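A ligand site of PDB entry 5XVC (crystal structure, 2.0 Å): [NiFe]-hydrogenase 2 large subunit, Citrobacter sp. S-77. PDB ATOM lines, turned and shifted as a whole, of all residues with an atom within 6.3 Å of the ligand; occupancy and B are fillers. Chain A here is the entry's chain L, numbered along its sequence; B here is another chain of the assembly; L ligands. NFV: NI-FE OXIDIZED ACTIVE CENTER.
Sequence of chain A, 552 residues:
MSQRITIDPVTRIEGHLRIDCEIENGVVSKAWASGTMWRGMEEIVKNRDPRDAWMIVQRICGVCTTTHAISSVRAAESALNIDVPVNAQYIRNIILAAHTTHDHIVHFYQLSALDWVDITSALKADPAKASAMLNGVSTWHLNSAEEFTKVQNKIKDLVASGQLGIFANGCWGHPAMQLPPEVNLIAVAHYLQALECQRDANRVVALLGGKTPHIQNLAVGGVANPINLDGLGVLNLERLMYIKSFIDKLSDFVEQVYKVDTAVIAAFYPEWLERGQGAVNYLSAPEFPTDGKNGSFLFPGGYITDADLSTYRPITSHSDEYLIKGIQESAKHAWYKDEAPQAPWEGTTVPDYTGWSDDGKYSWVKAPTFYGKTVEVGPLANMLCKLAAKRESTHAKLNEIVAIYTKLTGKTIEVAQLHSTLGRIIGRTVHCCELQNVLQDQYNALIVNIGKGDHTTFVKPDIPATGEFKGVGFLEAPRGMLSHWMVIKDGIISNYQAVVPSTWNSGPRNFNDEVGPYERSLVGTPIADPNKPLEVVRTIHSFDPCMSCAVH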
ATOM      1  N   GLU A  14      29.857   7.573  16.829  1.00  0.00           N
ATOM      2  CA  GLU A  14      29.309   6.801  15.723  1.00  0.00           C
ATOM      3  C   GLU A  14      27.812   7.082  15.626  1.00  0.00           C
ATOM      4  O   GLU A  14      27.074   7.043  16.619  1.00  0.00           O
ATOM      5  CB  GLU A  14      29.560   5.305  15.926  1.00  0.00           C
ATOM      6  CG  GLU A  14      29.263   4.447  14.699  1.00  0.00           C
ATOM      7  CD  GLU A  14      27.790   4.336  14.344  1.00  0.00           C
ATOM      8  OE1 GLU A  14      26.960   4.306  15.292  1.00  0.00           O
ATOM      9  OE2 GLU A  14      27.468   4.298  13.142  1.00  0.00           O
ATOM     10  N   ILE A  60      25.834  -4.454  12.640  1.00  0.00           N
ATOM     11  CA  ILE A  60      25.232  -3.474  13.537  1.00  0.00           C
ATOM     12  C   ILE A  60      26.171  -2.282  13.684  1.00  0.00           C
ATOM     13  O   ILE A  60      25.738  -1.111  13.667  1.00  0.00           O
ATOM     14  CB  ILE A  60      24.933  -4.083  14.896  1.00  0.00           C
ATOM     15  CG1 ILE A  60      23.681  -4.952  14.778  1.00  0.00           C
ATOM     16  CG2 ILE A  60      24.762  -2.979  15.959  1.00  0.00           C
ATOM     17  CD1 ILE A  60      23.363  -5.750  16.024  1.00  0.00           C
ATOM     18  N   CYS A  61      27.468  -2.567  13.759  1.00  0.00           N
ATOM     19  CA  CYS A  61      28.421  -1.484  13.866  1.00  0.00           C
ATOM     20  C   CYS A  61      29.820  -1.831  13.364  1.00  0.00           C
ATOM     21  O   CYS A  61      30.339  -2.918  13.627  1.00  0.00           O
ATOM     22  CB  CYS A  61      28.475  -0.990  15.305  1.00  0.00           C
ATOM     23  SG  CYS A  61      29.489   0.469  15.460  1.00  0.00           S
ATOM     24  N   GLY A  62      30.435  -0.894  12.665  1.00  0.00           N
ATOM     25  CA  GLY A  62      31.797  -1.081  12.153  1.00  0.00           C
ATOM     26  C   GLY A  62      32.877  -0.394  12.986  1.00  0.00           C
ATOM     27  O   GLY A  62      34.065  -0.547  12.699  1.00  0.00           O
ATOM     28  N   VAL A  63      32.477   0.378  13.993  1.00  0.00           N
ATOM     29  CA  VAL A  63      33.456   0.976  14.913  1.00  0.00           C
ATOM     30  C   VAL A  63      33.844  -0.124  15.866  1.00  0.00           C
ATOM     31  O   VAL A  63      35.015  -0.471  15.996  1.00  0.00           O
ATOM     32  CB  VAL A  63      32.856   2.142  15.756  1.00  0.00           C
ATOM     33  CG1 VAL A  63      33.914   2.737  16.712  1.00  0.00           C
ATOM     34  CG2 VAL A  63      32.322   3.210  14.863  1.00  0.00           C
ATOM     35  N   CYS A  64      32.848  -0.678  16.566  1.00  0.00           N
ATOM     36  CA  CYS A  64      33.084  -1.845  17.386  1.00  0.00           C
ATOM     37  C   CYS A  64      32.813  -3.070  16.522  1.00  0.00           C
ATOM     38  O   CYS A  64      32.015  -3.951  16.851  1.00  0.00           O
ATOM     39  CB  CYS A  64      32.217  -1.831  18.617  1.00  0.00           C
ATOM     40  SG  CYS A  64      30.488  -1.912  18.180  1.00  0.00           S
ATOM     41  N   THR A  65      33.500  -3.130  15.396  1.00  0.00           N
ATOM     42  CA  THR A  65      33.477  -4.309  14.579  1.00  0.00           C
ATOM     43  C   THR A  65      34.131  -5.418  15.413  1.00  0.00           C
ATOM     44  O   THR A  65      34.789  -5.114  16.417  1.00  0.00           O
ATOM     45  CB  THR A  65      34.194  -4.051  13.229  1.00  0.00           C
ATOM     46  OG1 THR A  65      34.060  -5.201  12.390  1.00  0.00           O
ATOM     47  CG2 THR A  65      35.673  -3.711  13.438  1.00  0.00           C
ATOM     48  N   THR A  67      32.692  -7.186  17.450  1.00  0.00           N
ATOM     49  CA  THR A  67      32.056  -7.280  18.741  1.00  0.00           C
ATOM     50  C   THR A  67      30.693  -8.025  18.658  1.00  0.00           C
ATOM     51  O   THR A  67      30.492  -9.063  19.296  1.00  0.00           O
ATOM     52  CB  THR A  67      32.027  -5.841  19.316  1.00  0.00           C
ATOM     53  OG1 THR A  67      32.707  -5.779  20.582  1.00  0.00           O
ATOM     54  CG2 THR A  67      30.697  -5.247  19.342  1.00  0.00           C
ATOM     55  N   HIS A  68      29.804  -7.545  17.794  1.00  0.00           N
ATOM     56  CA  HIS A  68      28.556  -8.229  17.537  1.00  0.00           C
ATOM     57  C   HIS A  68      28.788  -9.580  16.881  1.00  0.00           C
ATOM     58  O   HIS A  68      27.972 -10.478  17.025  1.00  0.00           O
ATOM     59  CB  HIS A  68      27.654  -7.349  16.680  1.00  0.00           C
ATOM     60  CG  HIS A  68      27.279  -6.066  17.351  1.00  0.00           C
ATOM     61  ND1 HIS A  68      26.348  -6.009  18.369  1.00  0.00           N
ATOM     62  CD2 HIS A  68      27.759  -4.810  17.198  1.00  0.00           C
ATOM     63  CE1 HIS A  68      26.252  -4.760  18.792  1.00  0.00           C
ATOM     64  NE2 HIS A  68      27.094  -4.019  18.107  1.00  0.00           N
ATOM     65  N   ASP A 103      40.163   0.708  19.192  1.00  0.00           N
ATOM     66  CA  ASP A 103      38.907   1.411  19.495  1.00  0.00           C
ATOM     67  C   ASP A 103      39.108   2.517  20.560  1.00  0.00           C
ATOM     68  O   ASP A 103      38.784   3.679  20.328  1.00  0.00           O
ATOM     69  CB  ASP A 103      37.822   0.411  19.924  1.00  0.00           C
ATOM     70  CG  ASP A 103      36.384   0.917  19.680  1.00  0.00           C
ATOM     71  OD1 ASP A 103      36.148   2.142  19.750  1.00  0.00           O
ATOM     72  OD2 ASP A 103      35.482   0.075  19.447  1.00  0.00           O
ATOM     73  N   LEU A 475      29.374 -10.462  25.994  1.00  0.00           N
ATOM     74  CA  LEU A 475      30.709 -10.006  25.639  1.00  0.00           C
ATOM     75  C   LEU A 475      30.975  -8.646  26.269  1.00  0.00           C
ATOM     76  O   LEU A 475      30.122  -7.761  26.239  1.00  0.00           O
ATOM     77  CB  LEU A 475      30.880  -9.956  24.104  1.00  0.00           C
ATOM     78  CG  LEU A 475      32.254  -9.556  23.515  1.00  0.00           C
ATOM     79  CD1 LEU A 475      32.496 -10.255  22.165  1.00  0.00           C
ATOM     80  CD2 LEU A 475      32.330  -8.057  23.313  1.00  0.00           C
ATOM     81  N   ALA A 477      32.416  -5.519  25.638  1.00  0.00           N
ATOM     82  CA  ALA A 477      32.852  -4.743  24.488  1.00  0.00           C
ATOM     83  C   ALA A 477      33.544  -3.466  24.951  1.00  0.00           C
ATOM     84  O   ALA A 477      33.429  -3.114  26.128  1.00  0.00           O
ATOM     85  CB  ALA A 477      31.639  -4.395  23.605  1.00  0.00           C
ATOM     86  N   PRO A 478      34.255  -2.793  24.037  1.00  0.00           N
ATOM     87  CA  PRO A 478      34.859  -1.493  24.358  1.00  0.00           C
ATOM     88  C   PRO A 478      33.927  -0.559  25.135  1.00  0.00           C
ATOM     89  O   PRO A 478      34.391   0.133  26.032  1.00  0.00           O
ATOM     90  CB  PRO A 478      35.139  -0.913  22.976  1.00  0.00           C
ATOM     91  CG  PRO A 478      35.526  -2.122  22.173  1.00  0.00           C
ATOM     92  CD  PRO A 478      34.588  -3.213  22.661  1.00  0.00           C
ATOM     93  N   ARG A 479      32.646  -0.555  24.798  1.00  0.00           N
ATOM     94  CA  ARG A 479      31.684   0.383  25.397  1.00  0.00           C
ATOM     95  C   ARG A 479      30.848  -0.245  26.538  1.00  0.00           C
ATOM     96  O   ARG A 479      30.034   0.437  27.148  1.00  0.00           O
ATOM     97  CB  ARG A 479      30.752   0.987  24.329  1.00  0.00           C
ATOM     98  CG  ARG A 479      31.428   2.073  23.469  1.00  0.00           C
ATOM     99  CD  ARG A 479      30.904   2.163  22.021  1.00  0.00           C
ATOM    100  NE  ARG A 479      31.833   2.984  21.250  1.00  0.00           N
ATOM    101  CZ  ARG A 479      32.911   2.497  20.622  1.00  0.00           C
ATOM    102  NH1 ARG A 479      33.153   1.186  20.654  1.00  0.00           N
ATOM    103  NH2 ARG A 479      33.742   3.315  19.985  1.00  0.00           N
ATOM    104  N   GLY A 480      31.057  -1.526  26.818  1.00  0.00           N
ATOM    105  CA  GLY A 480      30.370  -2.149  27.931  1.00  0.00           C
ATOM    106  C   GLY A 480      29.798  -3.530  27.621  1.00  0.00           C
ATOM    107  O   GLY A 480      30.100  -4.116  26.568  1.00  0.00           O
ATOM    108  N   LEU A 482      27.775  -6.363  26.328  1.00  0.00           N
ATOM    109  CA  LEU A 482      26.947  -6.587  25.151  1.00  0.00           C
ATOM    110  C   LEU A 482      26.318  -7.960  25.288  1.00  0.00           C
ATOM    111  O   LEU A 482      26.932  -8.872  25.850  1.00  0.00           O
ATOM    112  CB  LEU A 482      27.815  -6.501  23.887  1.00  0.00           C
ATOM    113  CG  LEU A 482      27.349  -7.104  22.564  1.00  0.00           C
ATOM    114  CD1 LEU A 482      26.135  -6.380  22.017  1.00  0.00           C
ATOM    115  CD2 LEU A 482      28.505  -7.139  21.528  1.00  0.00           C
ATOM    116  N   HIS A 484      23.727 -10.806  23.014  1.00  0.00           N
ATOM    117  CA  HIS A 484      22.902 -11.196  21.885  1.00  0.00           C
ATOM    118  C   HIS A 484      22.043 -12.358  22.320  1.00  0.00           C
ATOM    119  O   HIS A 484      22.519 -13.264  22.992  1.00  0.00           O
ATOM    120  CB  HIS A 484      23.768 -11.592  20.685  1.00  0.00           C
ATOM    121  CG  HIS A 484      24.249 -10.421  19.884  1.00  0.00           C
ATOM    122  ND1 HIS A 484      24.314 -10.427  18.512  1.00  0.00           N
ATOM    123  CD2 HIS A 484      24.693  -9.203  20.282  1.00  0.00           C
ATOM    124  CE1 HIS A 484      24.797  -9.265  18.091  1.00  0.00           C
ATOM    125  NE2 HIS A 484      25.031  -8.506  19.153  1.00  0.00           N
ATOM    126  N   VAL A 500      22.705  -3.790  23.625  1.00  0.00           N
ATOM    127  CA  VAL A 500      24.061  -3.344  23.307  1.00  0.00           C
ATOM    128  C   VAL A 500      24.469  -2.318  24.369  1.00  0.00           C
ATOM    129  O   VAL A 500      23.598  -1.647  24.926  1.00  0.00           O
ATOM    130  CB  VAL A 500      24.025  -2.752  21.879  1.00  0.00           C
ATOM    131  CG1 VAL A 500      25.429  -2.466  21.327  1.00  0.00           C
ATOM    132  CG2 VAL A 500      23.249  -3.724  20.952  1.00  0.00           C
ATOM    133  N   PRO A 501      25.773  -2.208  24.691  1.00  0.00           N
ATOM    134  CA  PRO A 501      26.130  -1.301  25.791  1.00  0.00           C
ATOM    135  C   PRO A 501      25.647   0.151  25.641  1.00  0.00           C
ATOM    136  O   PRO A 501      25.230   0.733  26.630  1.00  0.00           O
ATOM    137  CB  PRO A 501      27.667  -1.355  25.808  1.00  0.00           C
ATOM    138  CG  PRO A 501      28.067  -2.065  24.589  1.00  0.00           C
ATOM    139  CD  PRO A 501      26.947  -2.948  24.203  1.00  0.00           C
ATOM    140  N   SER A 502      25.717   0.737  24.443  1.00  0.00           N
ATOM    141  CA  SER A 502      25.180   2.075  24.257  1.00  0.00           C
ATOM    142  C   SER A 502      23.655   2.091  24.371  1.00  0.00           C
ATOM    143  O   SER A 502      23.057   3.169  24.513  1.00  0.00           O
ATOM    144  CB  SER A 502      25.619   2.719  22.937  1.00  0.00           C
ATOM    145  OG  SER A 502      26.994   3.106  22.970  1.00  0.00           O
ATOM    146  N   THR A 503      23.016   0.924  24.281  1.00  0.00           N
ATOM    147  CA  THR A 503      21.588   0.854  24.620  1.00  0.00           C
ATOM    148  C   THR A 503      21.420   1.132  26.121  1.00  0.00           C
ATOM    149  O   THR A 503      20.578   1.948  26.525  1.00  0.00           O
ATOM    150  CB  THR A 503      20.895  -0.489  24.219  1.00  0.00           C
ATOM    151  OG1 THR A 503      21.265  -0.857  22.865  1.00  0.00           O
ATOM    152  CG2 THR A 503      19.358  -0.374  24.296  1.00  0.00           C
ATOM    153  N   ASP A 544      31.540   7.365  25.161  1.00  0.00           N
ATOM    154  CA  ASP A 544      31.914   6.738  23.883  1.00  0.00           C
ATOM    155  C   ASP A 544      30.660   6.282  23.087  1.00  0.00           C
ATOM    156  O   ASP A 544      30.514   5.100  22.795  1.00  0.00           O
ATOM    157  CB  ASP A 544      32.858   5.562  24.166  1.00  0.00           C
ATOM    158  CG  ASP A 544      33.516   4.992  22.904  1.00  0.00           C
ATOM    159  OD1 ASP A 544      33.276   5.508  21.785  1.00  0.00           O
ATOM    160  OD2 ASP A 544      34.276   4.003  23.054  1.00  0.00           O
ATOM    161  N   PRO A 545      29.750   7.207  22.744  1.00  0.00           N
ATOM    162  CA  PRO A 545      28.462   6.799  22.172  1.00  0.00           C
ATOM    163  C   PRO A 545      28.576   6.128  20.812  1.00  0.00           C
ATOM    164  O   PRO A 545      29.385   6.546  19.953  1.00  0.00           O
ATOM    165  CB  PRO A 545      27.691   8.126  22.031  1.00  0.00           C
ATOM    166  CG  PRO A 545      28.329   9.035  22.979  1.00  0.00           C
ATOM    167  CD  PRO A 545      29.790   8.663  22.972  1.00  0.00           C
ATOM    168  N   CSO A 546      27.763   5.097  20.606  1.00  0.00           N
ATOM    169  CA  CSO A 546      27.684   4.457  19.303  1.00  0.00           C
ATOM    170  CB  CSO A 546      28.460   3.141  19.294  1.00  0.00           C
ATOM    171  SG  CSO A 546      28.461   2.534  17.568  1.00  0.00           S
ATOM    172  C   CSO A 546      26.220   4.222  19.034  1.00  0.00           C
ATOM    173  O   CSO A 546      25.594   3.378  19.672  1.00  0.00           O
ATOM    174  OD  CSO A 546      26.882   2.581  16.803  1.00  0.00           O
ATOM    175  N   MET A 547      25.641   4.975  18.108  1.00  0.00           N
ATOM    176  CA  MET A 547      24.184   4.956  17.954  1.00  0.00           C
ATOM    177  C   MET A 547      23.663   3.873  17.005  1.00  0.00           C
ATOM    178  O   MET A 547      22.513   3.474  17.076  1.00  0.00           O
ATOM    179  CB  MET A 547      23.656   6.352  17.582  1.00  0.00           C
ATOM    180  CG  MET A 547      24.027   7.425  18.620  1.00  0.00           C
ATOM    181  SD  MET A 547      23.710   6.952  20.349  1.00  0.00           S
ATOM    182  CE  MET A 547      21.912   6.804  20.310  1.00  0.00           C
ATOM    183  N   SER A 548      24.520   3.386  16.113  1.00  0.00           N
ATOM    184  CA  SER A 548      24.156   2.216  15.309  1.00  0.00           C
ATOM    185  C   SER A 548      24.114   1.010  16.235  1.00  0.00           C
ATOM    186  O   SER A 548      23.297   0.128  16.089  1.00  0.00           O
ATOM    187  CB  SER A 548      25.184   1.993  14.200  1.00  0.00           C
ATOM    188  OG  SER A 548      25.071   3.017  13.240  1.00  0.00           O
ATOM    189  N   CYS A 549      25.035   0.974  17.184  1.00  0.00           N
ATOM    190  CA  CYS A 549      24.986  -0.011  18.245  1.00  0.00           C
ATOM    191  C   CYS A 549      23.758   0.110  19.124  1.00  0.00           C
ATOM    192  O   CYS A 549      23.085  -0.877  19.410  1.00  0.00           O
ATOM    193  CB  CYS A 549      26.210   0.154  19.120  1.00  0.00           C
ATOM    194  SG  CYS A 549      27.443  -0.978  18.590  1.00  0.00           S
ATOM    195  N   ALA A 550      23.484   1.326  19.587  1.00  0.00           N
ATOM    196  CA  ALA A 550      22.377   1.571  20.521  1.00  0.00           C
ATOM    197  C   ALA A 550      21.018   1.185  19.921  1.00  0.00           C
ATOM    198  O   ALA A 550      20.136   0.649  20.606  1.00  0.00           O
ATOM    199  CB  ALA A 550      22.371   3.021  20.935  1.00  0.00           C
ATOM    200  N   CYS B  22      26.887   1.891   9.195  1.00  0.00           N
ATOM    201  CA  CYS B  22      27.411   1.272  10.419  1.00  0.00           C
ATOM    202  C   CYS B  22      28.750   1.895  10.801  1.00  0.00           C
ATOM    203  O   CYS B  22      29.337   1.556  11.836  1.00  0.00           O
ATOM    204  CB  CYS B  22      27.562  -0.256  10.263  1.00  0.00           C
ATOM    205  SG  CYS B  22      29.171  -0.849   9.560  1.00  0.00           S
HETATM  206 FE   NFV L   1      29.327  -1.169  20.257  1.00  0.00          FE
HETATM  207 NI   NFV L   1      29.562   0.543  17.780  1.00  0.00          NI
HETATM  208  C1  NFV L   1      28.871  -2.830  20.804  1.00  0.00           C
HETATM  209  O1  NFV L   1      28.593  -3.854  21.160  1.00  0.00           O
HETATM  210  C2  NFV L   1      28.336  -0.251  21.529  1.00  0.00           C
HETATM  211  N2  NFV L   1      27.767   0.281  22.276  1.00  0.00           N
HETATM  212  C3  NFV L   1      30.807  -1.236  21.378  1.00  0.00           C
HETATM  213  N3  NFV L   1      31.719  -1.297  22.114  1.00  0.00           N
HETATM  214  O4  NFV L   1      29.886   0.457  19.657  1.00  0.00           O
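SG of CSO 546 is bound to NI of the ligand, at 2.3 Å. The side-chain sulfur of Cys 61 is bound to a nickel atom (NI) of the ligand, 2.3 Å away. SG of Cys 64 is bound to FE of the ligand (2.5 Å). SG of Cys 549 binds FE of the ligand (2.5 Å). The backbone NH of Arg 479 is in hydrogen-bond range of a nitrogen (N3) of the ligand, at 2.9 Å. The guanidinium group (NH1) of Arg 479 is in hydrogen-bond range of a nitrogen (N3) of the ligand, 3.2 Å away. A nitrogen (N2) of the ligand lies within hydrogen-bond range of the backbone NH of Ser 502 (3.0 Å). OG of Ser 502 is in hydrogen-bond range of N2 of the ligand, at 3.0 Å. A ring nitrogen (NE2) of His 68 lies within hydrogen-bond range of an oxygen (O1) of the ligand, 3.4 Å away.
OG of Ser 502 is in hydrogen-bond range of N of CSO 546, 3.2 Å away. The backbone NH (N) of Ser 548 lies within hydrogen-bond range of OD of CSO 546, 2.6 Å away. The backbone NH of Val 63 lies close to the side-chain sulfur of Cys 61 (3.3 Å). SG of Cys 61 sits close to O of Cys 22 of chain B (3.8 Å). NE2 of His 68 lies close to SG of Cys 549. The side-chain carboxylate (OD1) of Asp 544 is in salt-bridge range of the guanidinium group (NH2) of Arg 479 (2.9 Å). A ring nitrogen (NE2) of His 484 lies within hydrogen-bond range of a ring nitrogen (ND1) of His 68, 2.9 Å away. The backbone carbonyl oxygen (O) of Val 500 lies close to the side-chain hydroxyl (OG1) of Thr 503 (3.2 Å).
CG2 of Thr 67 touches O1 of the ligand (3.1 Å). Ala 477 touches the ligand. Pro 478 touches the ligand. Leu 482 touches the ligand. CG1 of Val 500 touches O1 of the ligand, 3.5 Å away. Pro 501 touches the ligand. Hydrophobic or aromatic side chains within 4 Å of the ligand: His 68, Ala 477, Pro 478, Leu 482, Val 500 and Pro 501. Of the 29 residues printed, 13 come within 4 Å of the ligand. Along chain A the residues within 4 Å of the ligand span positions 61 to 549.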
